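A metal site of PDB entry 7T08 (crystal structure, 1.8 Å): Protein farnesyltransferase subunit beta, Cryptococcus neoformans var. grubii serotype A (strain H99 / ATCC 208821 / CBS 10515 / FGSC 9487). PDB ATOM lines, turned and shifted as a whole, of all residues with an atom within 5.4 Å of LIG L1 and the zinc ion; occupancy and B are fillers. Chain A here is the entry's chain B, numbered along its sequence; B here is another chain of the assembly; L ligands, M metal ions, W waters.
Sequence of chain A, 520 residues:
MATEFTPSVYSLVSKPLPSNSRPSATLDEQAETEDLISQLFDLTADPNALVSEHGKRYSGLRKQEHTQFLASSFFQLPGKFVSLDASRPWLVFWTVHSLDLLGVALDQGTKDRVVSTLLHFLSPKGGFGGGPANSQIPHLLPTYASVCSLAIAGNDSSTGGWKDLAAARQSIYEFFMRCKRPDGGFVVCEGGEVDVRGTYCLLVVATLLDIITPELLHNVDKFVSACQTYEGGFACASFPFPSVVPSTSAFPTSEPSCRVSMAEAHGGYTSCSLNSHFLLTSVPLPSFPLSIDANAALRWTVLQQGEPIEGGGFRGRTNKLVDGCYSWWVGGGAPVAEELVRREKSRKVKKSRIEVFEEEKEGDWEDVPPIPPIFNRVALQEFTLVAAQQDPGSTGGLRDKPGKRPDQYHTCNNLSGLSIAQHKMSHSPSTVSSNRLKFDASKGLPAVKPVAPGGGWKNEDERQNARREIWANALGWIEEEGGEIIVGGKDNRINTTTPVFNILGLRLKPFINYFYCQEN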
ATOM      1  N   LEU A  84     -12.337  -3.932 -22.850  1.00  0.00           N
ATOM      2  CA  LEU A  84     -11.364  -4.038 -23.926  1.00  0.00           C
ATOM      3  C   LEU A  84     -11.823  -3.337 -25.202  1.00  0.00           C
ATOM      4  O   LEU A  84     -11.258  -3.570 -26.281  1.00  0.00           O
ATOM      5  CB  LEU A  84     -11.053  -5.520 -24.209  1.00  0.00           C
ATOM      6  CG  LEU A  84     -10.276  -6.222 -23.088  1.00  0.00           C
ATOM      7  CD1 LEU A  84     -10.411  -7.739 -23.193  1.00  0.00           C
ATOM      8  CD2 LEU A  84      -8.820  -5.812 -23.122  1.00  0.00           C
ATOM      9  N   SER A  87      -9.251  -1.817 -27.253  1.00  0.00           N
ATOM     10  CA  SER A  87      -8.180  -2.724 -27.598  1.00  0.00           C
ATOM     11  C   SER A  87      -8.672  -3.804 -28.563  1.00  0.00           C
ATOM     12  O   SER A  87      -8.185  -4.933 -28.544  1.00  0.00           O
ATOM     13  CB  SER A  87      -7.592  -3.389 -26.345  1.00  0.00           C
ATOM     14  OG  SER A  87      -6.792  -2.466 -25.612  1.00  0.00           O
ATOM     15  N   TRP A  90      -6.215  -5.960 -30.421  1.00  0.00           N
ATOM     16  CA  TRP A  90      -5.593  -7.015 -29.612  1.00  0.00           C
ATOM     17  C   TRP A  90      -6.487  -8.260 -29.555  1.00  0.00           C
ATOM     18  O   TRP A  90      -5.979  -9.388 -29.586  1.00  0.00           O
ATOM     19  CB  TRP A  90      -5.325  -6.503 -28.192  1.00  0.00           C
ATOM     20  CG  TRP A  90      -4.194  -5.526 -28.162  1.00  0.00           C
ATOM     21  CD1 TRP A  90      -4.282  -4.159 -28.022  1.00  0.00           C
ATOM     22  CD2 TRP A  90      -2.802  -5.827 -28.306  1.00  0.00           C
ATOM     23  NE1 TRP A  90      -3.022  -3.598 -28.059  1.00  0.00           N
ATOM     24  CE2 TRP A  90      -2.097  -4.604 -28.236  1.00  0.00           C
ATOM     25  CE3 TRP A  90      -2.077  -7.010 -28.491  1.00  0.00           C
ATOM     26  CZ2 TRP A  90      -0.706  -4.527 -28.334  1.00  0.00           C
ATOM     27  CZ3 TRP A  90      -0.700  -6.930 -28.587  1.00  0.00           C
ATOM     28  CH2 TRP A  90      -0.022  -5.702 -28.512  1.00  0.00           C
ATOM     29  N   TRP A  94      -4.762 -11.670 -30.697  1.00  0.00           N
ATOM     30  CA  TRP A  94      -4.746 -12.824 -29.798  1.00  0.00           C
ATOM     31  C   TRP A  94      -5.453 -14.011 -30.436  1.00  0.00           C
ATOM     32  O   TRP A  94      -5.004 -15.156 -30.316  1.00  0.00           O
ATOM     33  CB  TRP A  94      -5.405 -12.483 -28.458  1.00  0.00           C
ATOM     34  CG  TRP A  94      -4.634 -11.432 -27.623  1.00  0.00           C
ATOM     35  CD1 TRP A  94      -3.284 -11.224 -27.599  1.00  0.00           C
ATOM     36  CD2 TRP A  94      -5.205 -10.470 -26.733  1.00  0.00           C
ATOM     37  NE1 TRP A  94      -2.984 -10.181 -26.728  1.00  0.00           N
ATOM     38  CE2 TRP A  94      -4.150  -9.716 -26.188  1.00  0.00           C
ATOM     39  CE3 TRP A  94      -6.521 -10.183 -26.339  1.00  0.00           C
ATOM     40  CZ2 TRP A  94      -4.361  -8.665 -25.269  1.00  0.00           C
ATOM     41  CZ3 TRP A  94      -6.730  -9.154 -25.426  1.00  0.00           C
ATOM     42  CH2 TRP A  94      -5.650  -8.406 -24.903  1.00  0.00           C
ATOM     43  N   LEU A 141      -0.050   0.902 -29.728  1.00  0.00           N
ATOM     44  CA  LEU A 141      -0.206  -0.512 -29.392  1.00  0.00           C
ATOM     45  C   LEU A 141      -1.196  -1.192 -30.331  1.00  0.00           C
ATOM     46  O   LEU A 141      -0.887  -2.269 -30.856  1.00  0.00           O
ATOM     47  CB  LEU A 141      -0.601  -0.661 -27.919  1.00  0.00           C
ATOM     48  CG  LEU A 141       0.542  -0.850 -26.913  1.00  0.00           C
ATOM     49  CD1 LEU A 141       1.522   0.319 -26.972  1.00  0.00           C
ATOM     50  CD2 LEU A 141      -0.012  -1.013 -25.494  1.00  0.00           C
ATOM     51  N   ARG A 197       6.770  -0.155 -24.040  1.00  0.00           N
ATOM     52  CA  ARG A 197       5.749  -0.798 -24.869  1.00  0.00           C
ATOM     53  C   ARG A 197       5.551  -0.024 -26.157  1.00  0.00           C
ATOM     54  O   ARG A 197       5.426  -0.613 -27.243  1.00  0.00           O
ATOM     55  CB  ARG A 197       4.395  -0.909 -24.126  1.00  0.00           C
ATOM     56  CG  ARG A 197       4.362  -1.796 -22.854  1.00  0.00           C
ATOM     57  CD  ARG A 197       3.054  -1.581 -22.067  1.00  0.00           C
ATOM     58  NE  ARG A 197       2.809  -0.134 -21.877  1.00  0.00           N
ATOM     59  CZ  ARG A 197       1.610   0.441 -21.966  1.00  0.00           C
ATOM     60  NH1 ARG A 197       0.517  -0.293 -22.201  1.00  0.00           N
ATOM     61  NH2 ARG A 197       1.501   1.757 -21.850  1.00  0.00           N
ATOM     62  N   ASP A 323       2.874 -17.153 -13.680  1.00  0.00           N
ATOM     63  CA  ASP A 323       1.696 -16.834 -14.489  1.00  0.00           C
ATOM     64  C   ASP A 323       1.996 -17.247 -15.922  1.00  0.00           C
ATOM     65  O   ASP A 323       3.059 -16.904 -16.461  1.00  0.00           O
ATOM     66  CB  ASP A 323       1.373 -15.313 -14.374  1.00  0.00           C
ATOM     67  CG  ASP A 323       0.283 -14.832 -15.342  1.00  0.00           C
ATOM     68  OD1 ASP A 323      -0.111 -15.560 -16.291  1.00  0.00           O
ATOM     69  OD2 ASP A 323      -0.182 -13.689 -15.167  1.00  0.00           O
ATOM     70  N   GLY A 324       1.066 -18.008 -16.536  1.00  0.00           N
ATOM     71  CA  GLY A 324       1.312 -18.562 -17.858  1.00  0.00           C
ATOM     72  C   GLY A 324       1.648 -17.538 -18.939  1.00  0.00           C
ATOM     73  O   GLY A 324       2.336 -17.869 -19.909  1.00  0.00           O
ATOM     74  N   CYS A 325       1.138 -16.309 -18.833  1.00  0.00           N
ATOM     75  CA  CYS A 325       1.445 -15.376 -19.931  1.00  0.00           C
ATOM     76  C   CYS A 325       2.925 -15.010 -19.986  1.00  0.00           C
ATOM     77  O   CYS A 325       3.411 -14.636 -21.069  1.00  0.00           O
ATOM     78  CB  CYS A 325       0.590 -14.097 -19.848  1.00  0.00           C
ATOM     79  SG  CYS A 325       0.874 -13.007 -18.395  1.00  0.00           S
ATOM     80  N   TYR A 326       3.663 -15.142 -18.887  1.00  0.00           N
ATOM     81  CA  TYR A 326       5.092 -14.861 -18.919  1.00  0.00           C
ATOM     82  C   TYR A 326       5.890 -15.949 -19.612  1.00  0.00           C
ATOM     83  O   TYR A 326       7.108 -15.784 -19.799  1.00  0.00           O
ATOM     84  CB  TYR A 326       5.611 -14.602 -17.479  1.00  0.00           C
ATOM     85  CG  TYR A 326       4.874 -13.417 -16.852  1.00  0.00           C
ATOM     86  CD1 TYR A 326       4.768 -12.204 -17.532  1.00  0.00           C
ATOM     87  CD2 TYR A 326       4.256 -13.527 -15.617  1.00  0.00           C
ATOM     88  CE1 TYR A 326       4.065 -11.130 -16.996  1.00  0.00           C
ATOM     89  CE2 TYR A 326       3.554 -12.440 -15.047  1.00  0.00           C
ATOM     90  CZ  TYR A 326       3.468 -11.249 -15.759  1.00  0.00           C
ATOM     91  OH  TYR A 326       2.792 -10.173 -15.240  1.00  0.00           O
ATOM     92  N   TRP A 329       6.402 -13.540 -22.422  1.00  0.00           N
ATOM     93  CA  TRP A 329       7.112 -12.302 -22.131  1.00  0.00           C
ATOM     94  C   TRP A 329       8.515 -12.573 -21.602  1.00  0.00           C
ATOM     95  O   TRP A 329       9.475 -11.897 -21.994  1.00  0.00           O
ATOM     96  CB  TRP A 329       6.321 -11.417 -21.148  1.00  0.00           C
ATOM     97  CG  TRP A 329       4.950 -11.055 -21.643  1.00  0.00           C
ATOM     98  CD1 TRP A 329       3.751 -11.415 -21.069  1.00  0.00           C
ATOM     99  CD2 TRP A 329       4.619 -10.307 -22.825  1.00  0.00           C
ATOM    100  NE1 TRP A 329       2.699 -10.922 -21.827  1.00  0.00           N
ATOM    101  CE2 TRP A 329       3.213 -10.241 -22.903  1.00  0.00           C
ATOM    102  CE3 TRP A 329       5.391  -9.685 -23.822  1.00  0.00           C
ATOM    103  CZ2 TRP A 329       2.544  -9.573 -23.948  1.00  0.00           C
ATOM    104  CZ3 TRP A 329       4.724  -9.009 -24.862  1.00  0.00           C
ATOM    105  CH2 TRP A 329       3.324  -8.972 -24.917  1.00  0.00           C
ATOM    106  N   ASP A 400      -4.015 -17.790 -16.585  1.00  0.00           N
ATOM    107  CA  ASP A 400      -2.898 -17.370 -15.745  1.00  0.00           C
ATOM    108  C   ASP A 400      -2.414 -18.518 -14.857  1.00  0.00           C
ATOM    109  O   ASP A 400      -1.253 -18.949 -14.952  1.00  0.00           O
ATOM    110  CB  ASP A 400      -3.375 -16.143 -14.930  1.00  0.00           C
ATOM    111  CG  ASP A 400      -2.594 -15.865 -13.647  1.00  0.00           C
ATOM    112  OD1 ASP A 400      -1.512 -16.433 -13.397  1.00  0.00           O
ATOM    113  OD2 ASP A 400      -3.092 -15.032 -12.861  1.00  0.00           O
ATOM    114  N   ASP A 407      -8.748 -16.587 -20.859  1.00  0.00           N
ATOM    115  CA  ASP A 407      -9.082 -15.436 -21.691  1.00  0.00           C
ATOM    116  C   ASP A 407      -8.204 -15.448 -22.922  1.00  0.00           C
ATOM    117  O   ASP A 407      -7.239 -16.220 -23.023  1.00  0.00           O
ATOM    118  CB  ASP A 407      -8.945 -14.116 -20.902  1.00  0.00           C
ATOM    119  CG  ASP A 407      -7.533 -13.876 -20.386  1.00  0.00           C
ATOM    120  OD1 ASP A 407      -6.591 -13.824 -21.196  1.00  0.00           O
ATOM    121  OD2 ASP A 407      -7.367 -13.704 -19.152  1.00  0.00           O
ATOM    122  N   GLN A 408      -8.542 -14.591 -23.888  1.00  0.00           N
ATOM    123  CA  GLN A 408      -7.831 -14.598 -25.162  1.00  0.00           C
ATOM    124  C   GLN A 408      -6.369 -14.179 -25.003  1.00  0.00           C
ATOM    125  O   GLN A 408      -5.498 -14.675 -25.731  1.00  0.00           O
ATOM    126  CB  GLN A 408      -8.519 -13.670 -26.162  1.00  0.00           C
ATOM    127  CG  GLN A 408      -9.928 -14.129 -26.569  1.00  0.00           C
ATOM    128  CD  GLN A 408     -10.994 -13.684 -25.588  1.00  0.00           C
ATOM    129  OE1 GLN A 408     -10.698 -13.196 -24.489  1.00  0.00           O
ATOM    130  NE2 GLN A 408     -12.251 -13.840 -25.987  1.00  0.00           N
ATOM    131  N   TYR A 409      -6.080 -13.277 -24.063  1.00  0.00           N
ATOM    132  CA  TYR A 409      -4.718 -12.803 -23.865  1.00  0.00           C
ATOM    133  C   TYR A 409      -3.829 -13.916 -23.306  1.00  0.00           C
ATOM    134  O   TYR A 409      -2.694 -14.104 -23.765  1.00  0.00           O
ATOM    135  CB  TYR A 409      -4.736 -11.570 -22.942  1.00  0.00           C
ATOM    136  CG  TYR A 409      -3.422 -11.280 -22.245  1.00  0.00           C
ATOM    137  CD1 TYR A 409      -2.444 -10.456 -22.837  1.00  0.00           C
ATOM    138  CD2 TYR A 409      -3.145 -11.825 -20.988  1.00  0.00           C
ATOM    139  CE1 TYR A 409      -1.223 -10.196 -22.182  1.00  0.00           C
ATOM    140  CE2 TYR A 409      -1.934 -11.575 -20.331  1.00  0.00           C
ATOM    141  CZ  TYR A 409      -0.984 -10.775 -20.929  1.00  0.00           C
ATOM    142  OH  TYR A 409       0.207 -10.563 -20.261  1.00  0.00           O
ATOM    143  N   HIS A 410      -4.315 -14.674 -22.315  1.00  0.00           N
ATOM    144  CA  HIS A 410      -3.529 -15.790 -21.798  1.00  0.00           C
ATOM    145  C   HIS A 410      -3.478 -16.958 -22.780  1.00  0.00           C
ATOM    146  O   HIS A 410      -2.525 -17.746 -22.755  1.00  0.00           O
ATOM    147  CB  HIS A 410      -4.067 -16.251 -20.440  1.00  0.00           C
ATOM    148  CG  HIS A 410      -3.690 -15.319 -19.323  1.00  0.00           C
ATOM    149  ND1 HIS A 410      -4.565 -14.384 -18.813  1.00  0.00           N
ATOM    150  CD2 HIS A 410      -2.523 -15.136 -18.674  1.00  0.00           C
ATOM    151  CE1 HIS A 410      -3.952 -13.687 -17.867  1.00  0.00           C
ATOM    152  NE2 HIS A 410      -2.705 -14.105 -17.778  1.00  0.00           N
ATOM    153  N   ASN A 413      -0.621 -15.844 -25.200  1.00  0.00           N
ATOM    154  CA  ASN A 413       0.738 -15.772 -24.665  1.00  0.00           C
ATOM    155  C   ASN A 413       1.215 -17.098 -24.072  1.00  0.00           C
ATOM    156  O   ASN A 413       2.412 -17.391 -24.170  1.00  0.00           O
ATOM    157  CB  ASN A 413       0.831 -14.610 -23.649  1.00  0.00           C
ATOM    158  CG  ASN A 413       0.872 -13.265 -24.357  1.00  0.00           C
ATOM    159  OD1 ASN A 413       1.798 -12.989 -25.105  1.00  0.00           O
ATOM    160  ND2 ASN A 413      -0.176 -12.463 -24.184  1.00  0.00           N
ATOM    161  N   TYR B 123      -3.904   2.119 -17.144  1.00  0.00           N
ATOM    162  CA  TYR B 123      -2.816   3.024 -17.534  1.00  0.00           C
ATOM    163  C   TYR B 123      -3.335   4.440 -17.753  1.00  0.00           C
ATOM    164  O   TYR B 123      -2.634   5.422 -17.460  1.00  0.00           O
ATOM    165  CB  TYR B 123      -2.137   2.560 -18.827  1.00  0.00           C
ATOM    166  CG  TYR B 123      -1.124   1.439 -18.736  1.00  0.00           C
ATOM    167  CD1 TYR B 123       0.241   1.712 -18.534  1.00  0.00           C
ATOM    168  CD2 TYR B 123      -1.505   0.120 -18.931  1.00  0.00           C
ATOM    169  CE1 TYR B 123       1.178   0.673 -18.513  1.00  0.00           C
ATOM    170  CE2 TYR B 123      -0.578  -0.916 -18.890  1.00  0.00           C
ATOM    171  CZ  TYR B 123       0.757  -0.638 -18.701  1.00  0.00           C
ATOM    172  OH  TYR B 123       1.668  -1.685 -18.693  1.00  0.00           O
HETATM  173  C1  LIG L   1      -4.770  -4.597 -23.695  1.00  0.00           C
HETATM  174  C2  LIG L   1      -3.952  -6.222 -17.950  1.00  0.00           C
HETATM  175  C3  LIG L   1      -2.521  -9.249 -16.645  1.00  0.00           C
HETATM  176  C4  LIG L   1      -8.191 -10.324 -21.320  1.00  0.00           C
HETATM  177  C5  LIG L   1      -7.669  -9.412 -20.186  1.00  0.00           C
HETATM  178  C6  LIG L   1      -6.134  -9.391 -20.097  1.00  0.00           C
HETATM  179  C7  LIG L   1      -5.613  -8.364 -19.024  1.00  0.00           C
HETATM  180  C8  LIG L   1      -3.995  -8.321 -18.991  1.00  0.00           C
HETATM  181  C9  LIG L   1      -3.537  -7.827 -20.342  1.00  0.00           C
HETATM  182  C10 LIG L   1      -3.695  -5.785 -21.914  1.00  0.00           C
HETATM  183  C11 LIG L   1      -4.810  -5.115 -22.400  1.00  0.00           C
HETATM  184  C12 LIG L   1      -3.643  -4.768 -24.481  1.00  0.00           C
HETATM  185  C13 LIG L   1      -2.526  -5.459 -24.000  1.00  0.00           C
HETATM  186  C14 LIG L   1      -0.495  -6.642 -24.601  1.00  0.00           C
HETATM  187  C15 LIG L   1      -2.564  -5.969 -22.699  1.00  0.00           C
HETATM  188  C16 LIG L   1      -3.935  -5.507 -19.368  1.00  0.00           C
HETATM  189  C17 LIG L   1      -3.547  -8.072 -16.759  1.00  0.00           C
HETATM  190  C18 LIG L   1      -2.805 -10.603 -16.833  1.00  0.00           C
HETATM  191  C19 LIG L   1      -0.686 -10.403 -16.374  1.00  0.00           C
HETATM  192  C20 LIG L   1      -0.437  -7.955 -16.050  1.00  0.00           C
HETATM  193  C21 LIG L   1      -0.339  -6.938 -17.230  1.00  0.00           C
HETATM  194  C22 LIG L   1      -0.417  -5.580 -16.986  1.00  0.00           C
HETATM  195  C23 LIG L   1      -0.313  -4.670 -18.042  1.00  0.00           C
HETATM  196  C24 LIG L   1      -0.122  -5.146 -19.344  1.00  0.00           C
HETATM  197  C25 LIG L   1      -0.006  -4.183 -20.526  1.00  0.00           C
HETATM  198  C26 LIG L   1      -0.040  -6.504 -19.571  1.00  0.00           C
HETATM  199  C27 LIG L   1      -0.145  -7.406 -18.527  1.00  0.00           C
HETATM  200  F1  LIG L   1      -1.155  -7.814 -24.427  1.00  0.00           F
HETATM  201  F2  LIG L   1       0.337  -6.728 -25.677  1.00  0.00           F
HETATM  202  F3  LIG L   1       0.266  -6.432 -23.489  1.00  0.00           F
HETATM  203  F4  LIG L   1       0.139  -6.963 -20.837  1.00  0.00           F
HETATM  204  N1  LIG L   1      -3.719  -6.360 -20.538  1.00  0.00           N
HETATM  205  N2  LIG L   1      -3.468  -7.523 -17.950  1.00  0.00           N
HETATM  206  N3  LIG L   1      -1.663 -11.283 -16.650  1.00  0.00           N
HETATM  207  N4  LIG L   1      -1.207  -9.182 -16.366  1.00  0.00           N
HETATM  208  N5  LIG L   1       0.089  -3.483 -21.424  1.00  0.00           N
HETATM  209  O1  LIG L   1      -1.401  -5.599 -24.833  1.00  0.00           O
HETATM  210  O2  LIG L   1      -4.092  -4.332 -19.487  1.00  0.00           O
HETATM  211  C1  LG2 L   2       2.123  -5.542 -13.684  1.00  0.00           C
HETATM  212  O1  LG2 L   2       0.813  -6.069 -13.597  1.00  0.00           O
HETATM  213  C2  LG2 L   2       2.561  -5.467 -15.157  1.00  0.00           C
HETATM  214  C3  LG2 L   2       2.704  -4.342 -15.861  1.00  0.00           C
HETATM  215  C4  LG2 L   2       2.432  -2.950 -15.249  1.00  0.00           C
HETATM  216  C5  LG2 L   2       3.141  -4.380 -17.332  1.00  0.00           C
HETATM  217  C6  LG2 L   2       3.255  -5.794 -17.945  1.00  0.00           C
HETATM  218  C7  LG2 L   2       3.420  -5.681 -19.477  1.00  0.00           C
HETATM  219  C8  LG2 L   2       3.302  -6.756 -20.273  1.00  0.00           C
HETATM  220  C9  LG2 L   2       3.035  -8.142 -19.678  1.00  0.00           C
HETATM  221  C10 LG2 L   2       3.453  -6.715 -21.801  1.00  0.00           C
HETATM  222  C11 LG2 L   2       3.552  -5.337 -22.473  1.00  0.00           C
HETATM  223  C12 LG2 L   2       3.913  -5.548 -23.962  1.00  0.00           C
HETATM  224  C13 LG2 L   2       3.270  -4.998 -25.010  1.00  0.00           C
HETATM  225  C14 LG2 L   2       3.764  -5.294 -26.433  1.00  0.00           C
HETATM  226  C15 LG2 L   2       2.073  -4.059 -24.843  1.00  0.00           C
HETATM  227  P1  LG2 L   2       0.356  -7.044 -12.343  1.00  0.00           P
HETATM  228  O2  LG2 L   2       0.779  -6.492 -11.004  1.00  0.00           O
HETATM  229  O3  LG2 L   2      -1.132  -7.234 -12.461  1.00  0.00           O
HETATM  230  O4  LG2 L   2       1.035  -8.517 -12.574  1.00  0.00           O
HETATM  231  P2  LG2 L   2       2.326  -9.191 -11.825  1.00  0.00           P
HETATM  232  O5  LG2 L   2       1.902  -9.504 -10.408  1.00  0.00           O
HETATM  233  O6  LG2 L   2       3.510  -8.266 -11.891  1.00  0.00           O
HETATM  234  O7  LG2 L   2       2.553 -10.471 -12.624  1.00  0.00           O
HETATM  235 ZN    ZN M   1      -0.978 -13.242 -16.988  1.00  0.00          ZN
HETATM  236  O   HOH W   1      -1.873  -9.910 -13.029  1.00  0.00           O
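The zinc ion is bound by OD2 of Asp 323, NE2 of His 410, N3 of LIG L1, SG of Cys 325 and OD1 of Asp 323. The zinc ion has five donor atoms within binding distance.
OH of Tyr 326 sits at hydrogen-bond distance from O7 of LG2 L2 (2.6 Å). NH1 of Arg 197 is in hydrogen-bond range of N5 of LIG L1 (3.3 Å).
Merely in contact with the zinc ion: Tyr 409. Within 4 Å of the zinc ion: Asp 323, Cys 325, Tyr 409 and His 410.
OH of Tyr 409 sits close to SG of Cys 325 (3.1 Å). The side-chain hydroxyl (OH) of Tyr 409 sits at hydrogen-bond distance from the indole nitrogen (NE1) of Trp 329 (3.0 Å). The backbone NH (N) of His 410 sits at hydrogen-bond distance from the side-chain carboxylate (OD1) of Asp 407, at 2.7 Å. The side-chain carboxylate (OD1) of Asp 407 lies within hydrogen-bond range of the backbone NH (N) of Tyr 409 (3.0 Å). The backbone carbonyl oxygen of Tyr 409 is in hydrogen-bond range of the side-chain amide nitrogen of Asn 413 (3.0 Å).
Residues that only touch LIG L1: Leu 84, Ser 87, Trp 90, Trp 94, Tyr 326, Trp 329, Asp 407, Tyr 409 and Tyr 123 of chain B. Hydrophobic or aromatic side chains that line LIG L1: Leu 84, Trp 90, Trp 94, Trp 329, Tyr 409, His 410 and Tyr 123 of chain B. The nearest printed residue that does not touch LIG L1 is Asn 413 (4.8 Å).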
